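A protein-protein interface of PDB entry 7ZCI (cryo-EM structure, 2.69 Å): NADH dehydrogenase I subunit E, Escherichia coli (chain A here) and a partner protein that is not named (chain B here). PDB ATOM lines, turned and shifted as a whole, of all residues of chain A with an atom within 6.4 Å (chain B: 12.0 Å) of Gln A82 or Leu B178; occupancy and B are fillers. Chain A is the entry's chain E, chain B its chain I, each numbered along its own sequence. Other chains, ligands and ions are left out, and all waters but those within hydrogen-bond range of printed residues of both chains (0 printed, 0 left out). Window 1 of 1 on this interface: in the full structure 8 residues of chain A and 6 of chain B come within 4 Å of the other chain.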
ATOM      1  N   GLY A  48      -6.393  11.338 -11.125  1.00  0.00           N
ATOM      2  CA  GLY A  48      -6.554  11.232  -9.682  1.00  0.00           C
ATOM      3  C   GLY A  48      -5.358  10.652  -8.961  1.00  0.00           C
ATOM      4  O   GLY A  48      -5.035  11.072  -7.850  1.00  0.00           O
ATOM      5  N   TRP A  49      -4.695   9.682  -9.582  1.00  0.00           N
ATOM      6  CA  TRP A  49      -3.550   8.997  -9.004  1.00  0.00           C
ATOM      7  C   TRP A  49      -2.733   8.423 -10.148  1.00  0.00           C
ATOM      8  O   TRP A  49      -3.155   8.446 -11.304  1.00  0.00           O
ATOM      9  CB  TRP A  49      -3.982   7.898  -8.027  1.00  0.00           C
ATOM     10  CG  TRP A  49      -4.688   6.746  -8.674  1.00  0.00           C
ATOM     11  CD1 TRP A  49      -5.878   6.780  -9.329  1.00  0.00           C
ATOM     12  CD2 TRP A  49      -4.248   5.384  -8.718  1.00  0.00           C
ATOM     13  NE1 TRP A  49      -6.206   5.530  -9.786  1.00  0.00           N
ATOM     14  CE2 TRP A  49      -5.220   4.655  -9.422  1.00  0.00           C
ATOM     15  CE3 TRP A  49      -3.123   4.714  -8.234  1.00  0.00           C
ATOM     16  CZ2 TRP A  49      -5.103   3.290  -9.652  1.00  0.00           C
ATOM     17  CZ3 TRP A  49      -3.012   3.358  -8.462  1.00  0.00           C
ATOM     18  CH2 TRP A  49      -3.994   2.662  -9.165  1.00  0.00           C
ATOM     19  N   VAL A  50      -1.556   7.905  -9.812  1.00  0.00           N
ATOM     20  CA  VAL A  50      -0.638   7.333 -10.791  1.00  0.00           C
ATOM     21  C   VAL A  50      -0.789   5.815 -10.737  1.00  0.00           C
ATOM     22  O   VAL A  50      -0.357   5.197  -9.752  1.00  0.00           O
ATOM     23  CB  VAL A  50       0.809   7.757 -10.514  1.00  0.00           C
ATOM     24  CG1 VAL A  50       1.748   7.133 -11.520  1.00  0.00           C
ATOM     25  CG2 VAL A  50       0.930   9.266 -10.525  1.00  0.00           C
ATOM     26  N   SER A  77       5.241  12.162  -1.051  1.00  0.00           N
ATOM     27  CA  SER A  77       3.985  11.846  -0.386  1.00  0.00           C
ATOM     28  C   SER A  77       2.780  12.276  -1.209  1.00  0.00           C
ATOM     29  O   SER A  77       1.724  11.643  -1.128  1.00  0.00           O
ATOM     30  CB  SER A  77       3.948  12.504   0.989  1.00  0.00           C
ATOM     31  OG  SER A  77       4.416  13.835   0.923  1.00  0.00           O
ATOM     32  N   ILE A  79       2.432  12.265  -4.469  1.00  0.00           N
ATOM     33  CA  ILE A  79       2.198  11.448  -5.653  1.00  0.00           C
ATOM     34  C   ILE A  79       1.556  10.153  -5.179  1.00  0.00           C
ATOM     35  O   ILE A  79       2.177   9.367  -4.459  1.00  0.00           O
ATOM     36  CB  ILE A  79       3.490  11.193  -6.438  1.00  0.00           C
ATOM     37  CG1 ILE A  79       3.974  12.497  -7.064  1.00  0.00           C
ATOM     38  CG2 ILE A  79       3.258  10.161  -7.524  1.00  0.00           C
ATOM     39  CD1 ILE A  79       5.377  12.438  -7.576  1.00  0.00           C
ATOM     40  N   PHE A  80       0.304   9.939  -5.565  1.00  0.00           N
ATOM     41  CA  PHE A  80      -0.507   8.863  -5.014  1.00  0.00           C
ATOM     42  C   PHE A  80      -0.381   7.624  -5.884  1.00  0.00           C
ATOM     43  O   PHE A  80      -0.749   7.641  -7.062  1.00  0.00           O
ATOM     44  CB  PHE A  80      -1.966   9.294  -4.896  1.00  0.00           C
ATOM     45  CG  PHE A  80      -2.169  10.480  -4.009  1.00  0.00           C
ATOM     46  CD1 PHE A  80      -1.473  10.595  -2.821  1.00  0.00           C
ATOM     47  CD2 PHE A  80      -3.043  11.486  -4.364  1.00  0.00           C
ATOM     48  CE1 PHE A  80      -1.653  11.680  -2.005  1.00  0.00           C
ATOM     49  CE2 PHE A  80      -3.221  12.576  -3.549  1.00  0.00           C
ATOM     50  CZ  PHE A  80      -2.527  12.672  -2.370  1.00  0.00           C
ATOM     51  N   ARG A  81       0.128   6.549  -5.296  1.00  0.00           N
ATOM     52  CA  ARG A  81       0.325   5.289  -5.991  1.00  0.00           C
ATOM     53  C   ARG A  81      -0.761   4.279  -5.656  1.00  0.00           C
ATOM     54  O   ARG A  81      -0.654   3.111  -6.036  1.00  0.00           O
ATOM     55  CB  ARG A  81       1.709   4.739  -5.660  1.00  0.00           C
ATOM     56  CG  ARG A  81       2.813   5.288  -6.539  1.00  0.00           C
ATOM     57  CD  ARG A  81       2.550   4.991  -7.990  1.00  0.00           C
ATOM     58  NE  ARG A  81       3.120   3.701  -8.347  1.00  0.00           N
ATOM     59  CZ  ARG A  81       2.421   2.671  -8.797  1.00  0.00           C
ATOM     60  NH1 ARG A  81       1.124   2.764  -9.027  1.00  0.00           N
ATOM     61  NH2 ARG A  81       3.040   1.517  -9.017  1.00  0.00           N
ATOM     62  N   GLN A  82      -1.801   4.706  -4.954  1.00  0.00           N
ATOM     63  CA  GLN A  82      -2.997   3.937  -4.664  1.00  0.00           C
ATOM     64  C   GLN A  82      -4.207   4.776  -5.037  1.00  0.00           C
ATOM     65  O   GLN A  82      -4.110   6.005  -5.079  1.00  0.00           O
ATOM     66  CB  GLN A  82      -3.063   3.547  -3.181  1.00  0.00           C
ATOM     67  CG  GLN A  82      -2.312   2.283  -2.855  1.00  0.00           C
ATOM     68  CD  GLN A  82      -2.172   2.064  -1.372  1.00  0.00           C
ATOM     69  OE1 GLN A  82      -2.511   2.932  -0.571  1.00  0.00           O
ATOM     70  NE2 GLN A  82      -1.657   0.902  -0.993  1.00  0.00           N
ATOM     71  N   PRO A  83      -5.338   4.148  -5.361  1.00  0.00           N
ATOM     72  CA  PRO A  83      -6.519   4.930  -5.745  1.00  0.00           C
ATOM     73  C   PRO A  83      -7.047   5.779  -4.599  1.00  0.00           C
ATOM     74  O   PRO A  83      -7.202   5.312  -3.469  1.00  0.00           O
ATOM     75  CB  PRO A  83      -7.534   3.861  -6.165  1.00  0.00           C
ATOM     76  CG  PRO A  83      -7.021   2.591  -5.595  1.00  0.00           C
ATOM     77  CD  PRO A  83      -5.544   2.713  -5.610  1.00  0.00           C
ATOM     78  N   VAL A  84      -7.315   7.044  -4.908  1.00  0.00           N
ATOM     79  CA  VAL A  84      -7.861   7.988  -3.942  1.00  0.00           C
ATOM     80  C   VAL A  84      -9.303   8.289  -4.317  1.00  0.00           C
ATOM     81  O   VAL A  84      -9.794   7.835  -5.355  1.00  0.00           O
ATOM     82  CB  VAL A  84      -7.026   9.278  -3.886  1.00  0.00           C
ATOM     83  CG1 VAL A  84      -5.708   9.022  -3.196  1.00  0.00           C
ATOM     84  CG2 VAL A  84      -6.798   9.816  -5.278  1.00  0.00           C
ATOM     85  N   GLY A 118      -5.966   8.096   5.920  1.00  0.00           N
ATOM     86  CA  GLY A 118      -5.435   7.175   4.943  1.00  0.00           C
ATOM     87  C   GLY A 118      -6.466   6.317   4.248  1.00  0.00           C
ATOM     88  O   GLY A 118      -6.095   5.498   3.400  1.00  0.00           O
ATOM     89  N   GLN A 119      -7.741   6.474   4.576  1.00  0.00           N
ATOM     90  CA  GLN A 119      -8.812   5.677   4.004  1.00  0.00           C
ATOM     91  C   GLN A 119      -9.696   6.537   3.113  1.00  0.00           C
ATOM     92  O   GLN A 119      -9.672   7.767   3.173  1.00  0.00           O
ATOM     93  CB  GLN A 119      -9.657   5.028   5.102  1.00  0.00           C
ATOM     94  CG  GLN A 119      -9.262   3.608   5.427  1.00  0.00           C
ATOM     95  CD  GLN A 119      -9.811   3.149   6.756  1.00  0.00           C
ATOM     96  OE1 GLN A 119     -10.989   3.332   7.050  1.00  0.00           O
ATOM     97  NE2 GLN A 119      -8.957   2.547   7.571  1.00  0.00           N
ATOM     98  N   THR A 120     -10.482   5.861   2.282  1.00  0.00           N
ATOM     99  CA  THR A 120     -11.415   6.494   1.364  1.00  0.00           C
ATOM    100  C   THR A 120     -12.825   6.064   1.741  1.00  0.00           C
ATOM    101  O   THR A 120     -13.043   4.916   2.138  1.00  0.00           O
ATOM    102  CB  THR A 120     -11.100   6.101  -0.090  1.00  0.00           C
ATOM    103  OG1 THR A 120      -9.725   6.380  -0.371  1.00  0.00           O
ATOM    104  CG2 THR A 120     -11.961   6.872  -1.078  1.00  0.00           C
ATOM    105  N   THR A 127     -11.024  11.168   0.490  1.00  0.00           N
ATOM    106  CA  THR A 127      -9.969  10.414   1.147  1.00  0.00           C
ATOM    107  C   THR A 127      -9.276  11.336   2.139  1.00  0.00           C
ATOM    108  O   THR A 127      -8.929  12.470   1.805  1.00  0.00           O
ATOM    109  CB  THR A 127      -8.987   9.811   0.130  1.00  0.00           C
ATOM    110  OG1 THR A 127      -7.852   9.261   0.806  1.00  0.00           O
ATOM    111  CG2 THR A 127      -8.547  10.825  -0.890  1.00  0.00           C
ATOM    112  N   LEU A 129      -6.343  12.476   4.733  1.00  0.00           N
ATOM    113  CA  LEU A 129      -4.913  12.357   4.866  1.00  0.00           C
ATOM    114  C   LEU A 129      -4.385  13.430   5.806  1.00  0.00           C
ATOM    115  O   LEU A 129      -4.795  14.599   5.719  1.00  0.00           O
ATOM    116  CB  LEU A 129      -4.209  12.485   3.509  1.00  0.00           C
ATOM    117  CG  LEU A 129      -4.352  11.329   2.523  1.00  0.00           C
ATOM    118  CD1 LEU A 129      -3.645  11.647   1.225  1.00  0.00           C
ATOM    119  CD2 LEU A 129      -3.814  10.049   3.122  1.00  0.00           C
ATOM    120  N   PRO A 130      -3.488  13.057   6.718  1.00  0.00           N
ATOM    121  CA  PRO A 130      -2.712  14.054   7.460  1.00  0.00           C
ATOM    122  C   PRO A 130      -1.536  14.512   6.612  1.00  0.00           C
ATOM    123  O   PRO A 130      -0.772  13.697   6.095  1.00  0.00           O
ATOM    124  CB  PRO A 130      -2.249  13.288   8.703  1.00  0.00           C
ATOM    125  CG  PRO A 130      -2.219  11.867   8.277  1.00  0.00           C
ATOM    126  CD  PRO A 130      -3.209  11.684   7.168  1.00  0.00           C
ATOM    127  N   LYS B 171       2.525  -4.815  11.076  1.00  0.00           N
ATOM    128  CA  LYS B 171       2.073  -5.265   9.773  1.00  0.00           C
ATOM    129  C   LYS B 171       2.879  -4.573   8.675  1.00  0.00           C
ATOM    130  O   LYS B 171       3.317  -3.434   8.846  1.00  0.00           O
ATOM    131  CB  LYS B 171       0.583  -4.976   9.595  1.00  0.00           C
ATOM    132  CG  LYS B 171      -0.374  -6.156   9.823  1.00  0.00           C
ATOM    133  CD  LYS B 171      -0.017  -7.102  10.978  1.00  0.00           C
ATOM    134  CE  LYS B 171      -0.078  -6.434  12.360  1.00  0.00           C
ATOM    135  NZ  LYS B 171       0.558  -7.263  13.421  1.00  0.00           N
ATOM    136  N   PRO B 172       3.115  -5.253   7.553  1.00  0.00           N
ATOM    137  CA  PRO B 172       3.923  -4.653   6.480  1.00  0.00           C
ATOM    138  C   PRO B 172       3.197  -3.492   5.817  1.00  0.00           C
ATOM    139  O   PRO B 172       2.127  -3.659   5.232  1.00  0.00           O
ATOM    140  CB  PRO B 172       4.144  -5.817   5.508  1.00  0.00           C
ATOM    141  CG  PRO B 172       3.074  -6.781   5.811  1.00  0.00           C
ATOM    142  CD  PRO B 172       2.782  -6.657   7.264  1.00  0.00           C
ATOM    143  N   ILE B 173       3.780  -2.306   5.935  1.00  0.00           N
ATOM    144  CA  ILE B 173       3.260  -1.125   5.255  1.00  0.00           C
ATOM    145  C   ILE B 173       3.724  -1.173   3.810  1.00  0.00           C
ATOM    146  O   ILE B 173       4.927  -1.182   3.539  1.00  0.00           O
ATOM    147  CB  ILE B 173       3.734   0.164   5.936  1.00  0.00           C
ATOM    148  CG1 ILE B 173       3.270   0.210   7.385  1.00  0.00           C
ATOM    149  CG2 ILE B 173       3.248   1.371   5.168  1.00  0.00           C
ATOM    150  CD1 ILE B 173       3.949   1.276   8.188  1.00  0.00           C
ATOM    151  N   ASP B 174       2.774  -1.208   2.881  1.00  0.00           N
ATOM    152  CA  ASP B 174       3.132  -1.195   1.473  1.00  0.00           C
ATOM    153  C   ASP B 174       3.739   0.148   1.103  1.00  0.00           C
ATOM    154  O   ASP B 174       3.337   1.199   1.603  1.00  0.00           O
ATOM    155  CB  ASP B 174       1.920  -1.477   0.591  1.00  0.00           C
ATOM    156  CG  ASP B 174       2.311  -2.031  -0.762  1.00  0.00           C
ATOM    157  OD1 ASP B 174       2.811  -1.257  -1.600  1.00  0.00           O
ATOM    158  OD2 ASP B 174       2.129  -3.243  -0.988  1.00  0.00           O
ATOM    159  N   VAL B 175       4.729   0.097   0.215  1.00  0.00           N
ATOM    160  CA  VAL B 175       5.506   1.277  -0.121  1.00  0.00           C
ATOM    161  C   VAL B 175       4.677   2.292  -0.901  1.00  0.00           C
ATOM    162  O   VAL B 175       5.017   3.477  -0.930  1.00  0.00           O
ATOM    163  CB  VAL B 175       6.773   0.811  -0.869  1.00  0.00           C
ATOM    164  CG1 VAL B 175       6.722   1.115  -2.358  1.00  0.00           C
ATOM    165  CG2 VAL B 175       7.998   1.349  -0.213  1.00  0.00           C
ATOM    166  N   LYS B 176       3.563   1.855  -1.488  1.00  0.00           N
ATOM    167  CA  LYS B 176       2.649   2.699  -2.235  1.00  0.00           C
ATOM    168  C   LYS B 176       1.517   3.246  -1.378  1.00  0.00           C
ATOM    169  O   LYS B 176       0.498   3.676  -1.924  1.00  0.00           O
ATOM    170  CB  LYS B 176       2.074   1.919  -3.416  1.00  0.00           C
ATOM    171  CG  LYS B 176       3.131   1.323  -4.316  1.00  0.00           C
ATOM    172  CD  LYS B 176       2.533   0.744  -5.579  1.00  0.00           C
ATOM    173  CE  LYS B 176       1.410  -0.224  -5.287  1.00  0.00           C
ATOM    174  NZ  LYS B 176       1.643  -1.531  -5.950  1.00  0.00           N
ATOM    175  N   SER B 177       1.662   3.228  -0.058  1.00  0.00           N
ATOM    176  CA  SER B 177       0.597   3.689   0.819  1.00  0.00           C
ATOM    177  C   SER B 177       0.457   5.204   0.757  1.00  0.00           C
ATOM    178  O   SER B 177       1.428   5.933   0.550  1.00  0.00           O
ATOM    179  CB  SER B 177       0.861   3.257   2.258  1.00  0.00           C
ATOM    180  OG  SER B 177       2.038   3.861   2.753  1.00  0.00           O
ATOM    181  N   LEU B 178      -0.779   5.672   0.948  1.00  0.00           N
ATOM    182  CA  LEU B 178      -1.066   7.097   0.851  1.00  0.00           C
ATOM    183  C   LEU B 178      -0.519   7.876   2.035  1.00  0.00           C
ATOM    184  O   LEU B 178      -0.265   9.078   1.917  1.00  0.00           O
ATOM    185  CB  LEU B 178      -2.572   7.321   0.743  1.00  0.00           C
ATOM    186  CG  LEU B 178      -3.281   6.578  -0.382  1.00  0.00           C
ATOM    187  CD1 LEU B 178      -4.781   6.705  -0.236  1.00  0.00           C
ATOM    188  CD2 LEU B 178      -2.818   7.122  -1.712  1.00  0.00           C
ATOM    189  N   LEU B 179      -0.349   7.221   3.175  1.00  0.00           N
ATOM    190  CA  LEU B 179       0.070   7.915   4.381  1.00  0.00           C
ATOM    191  C   LEU B 179       1.531   8.343   4.269  1.00  0.00           C
ATOM    192  O   LEU B 179       2.348   7.617   3.699  1.00  0.00           O
ATOM    193  CB  LEU B 179      -0.126   7.017   5.597  1.00  0.00           C
ATOM    194  CG  LEU B 179      -1.582   6.836   6.025  1.00  0.00           C
ATOM    195  CD1 LEU B 179      -1.708   5.731   7.047  1.00  0.00           C
ATOM    196  CD2 LEU B 179      -2.120   8.132   6.580  1.00  0.00           C
ATOM    197  N   PRO B 180       1.891   9.523   4.796  1.00  0.00           N
ATOM    198  CA  PRO B 180       3.270  10.021   4.757  1.00  0.00           C
ATOM    199  C   PRO B 180       4.244   9.175   5.578  1.00  0.00           C
ATOM    200  O   PRO B 180       3.835   8.558   6.563  1.00  0.00           O
ATOM    201  CB  PRO B 180       3.151  11.425   5.355  1.00  0.00           C
ATOM    202  CG  PRO B 180       1.730  11.779   5.227  1.00  0.00           C
ATOM    203  CD  PRO B 180       0.975  10.513   5.381  1.00  0.00           C
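O of Val A50 lies within hydrogen-bond range of NH1 of Arg A81 (2.9 Å). The backbone carbonyl oxygen (O) of Asp B174 lies within hydrogen-bond range of the side-chain hydroxyl (OG) of Ser B177. O of Phe A80 sits at hydrogen-bond distance from N of Val A50. The side-chain carboxylate of Asp B174 sits close to the backbone NH of Lys B176 (3.2 Å).
The backbone carbonyl oxygen of Lys B176 sits close to the side-chain amide oxygen of Gln A82 (3.4 Å).
Of the 16 printed residues of chain A, 7 touch a printed residue of chain B. Printed residues of chain A that touch a printed residue of chain B: Phe A80, Arg A81, Gln A82, Val A84, Gly A118, Leu A129 and Pro A130. Hydrophobic or aromatic side chains of chain A that line the printed part of chain B: Phe A80, Val A84, Leu A129 and Pro A130. Hydrophobic or aromatic side chains of chain B within 4 Å of the printed part of chain A: Leu B178, Leu B179 and Pro B180. Among the printed residues, 10 pairs touch across the chains. Among the printed residues, no Asp or Glu carboxylate lies within 4 Å of a Lys or Arg side-chain nitrogen of the other chain.
No residue of chain B comes within 4 Å of Val A50. No residue of chain B comes within 4 Å of Ser A77. Phe A80 touches just one residue of chain B: Leu B178 (3.9 Å). Arg A81 touches one residue of chain B. Of chain B, only Lys B176, Ser B177 and Leu B178 come within 4 Å of Gln A82. Of the printed residues of chain B, Val A84 touches Leu B178 (3.8 Å). Of chain B, only Leu B179 comes within 4 Å of Gly A118. No residue of chain B comes within 4 Å of Thr A127. Of the printed residues of chain B, Leu A129 touches Leu B178 (3.8 Å). Of the printed residues of chain A, Lys B176 touches Arg A81 and Gln A82. Printed residues of chain A within 4 Å of Ser B177: Gln A82. Of chain A, only Phe A80, Gln A82, Val A84 and Leu A129 come within 4 Å of Leu B178. Printed residues of chain A within 4 Å of Leu B179: Gly A118 and Pro A130. Printed residues of chain A within 4 Å of Pro B180: Pro A130 (3.3 Å). The nearest residue of chain B that does not touch Gln A82 is Asp B174 (4.6 Å). The nearest residue of chain A that does not touch Leu B178 is Gly A118 (4.1 Å). The nearest printed residue of chain A that does not touch Ser B177 is Arg A81 (5.8 Å).
Leu B178 touches Phe A80. Arg A81 touches Lys B176 (NH2 to CD, 3.6 Å). Ser B177 touches Gln A82 (CA to OE1, 3.5 Å). Gln A82 touches Leu B178. CD2 of Leu B178 touches CG1 of Val A84, at 3.8 Å. CA of Gly A118 touches CD2 of Leu B179, 3.8 Å away. Leu A129 touches Leu B178 (CD2 to CB, 3.8 Å). Pro A130 touches Leu B179 (CD to CD2, 3.8 Å). Pro A130 touches Pro B180.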
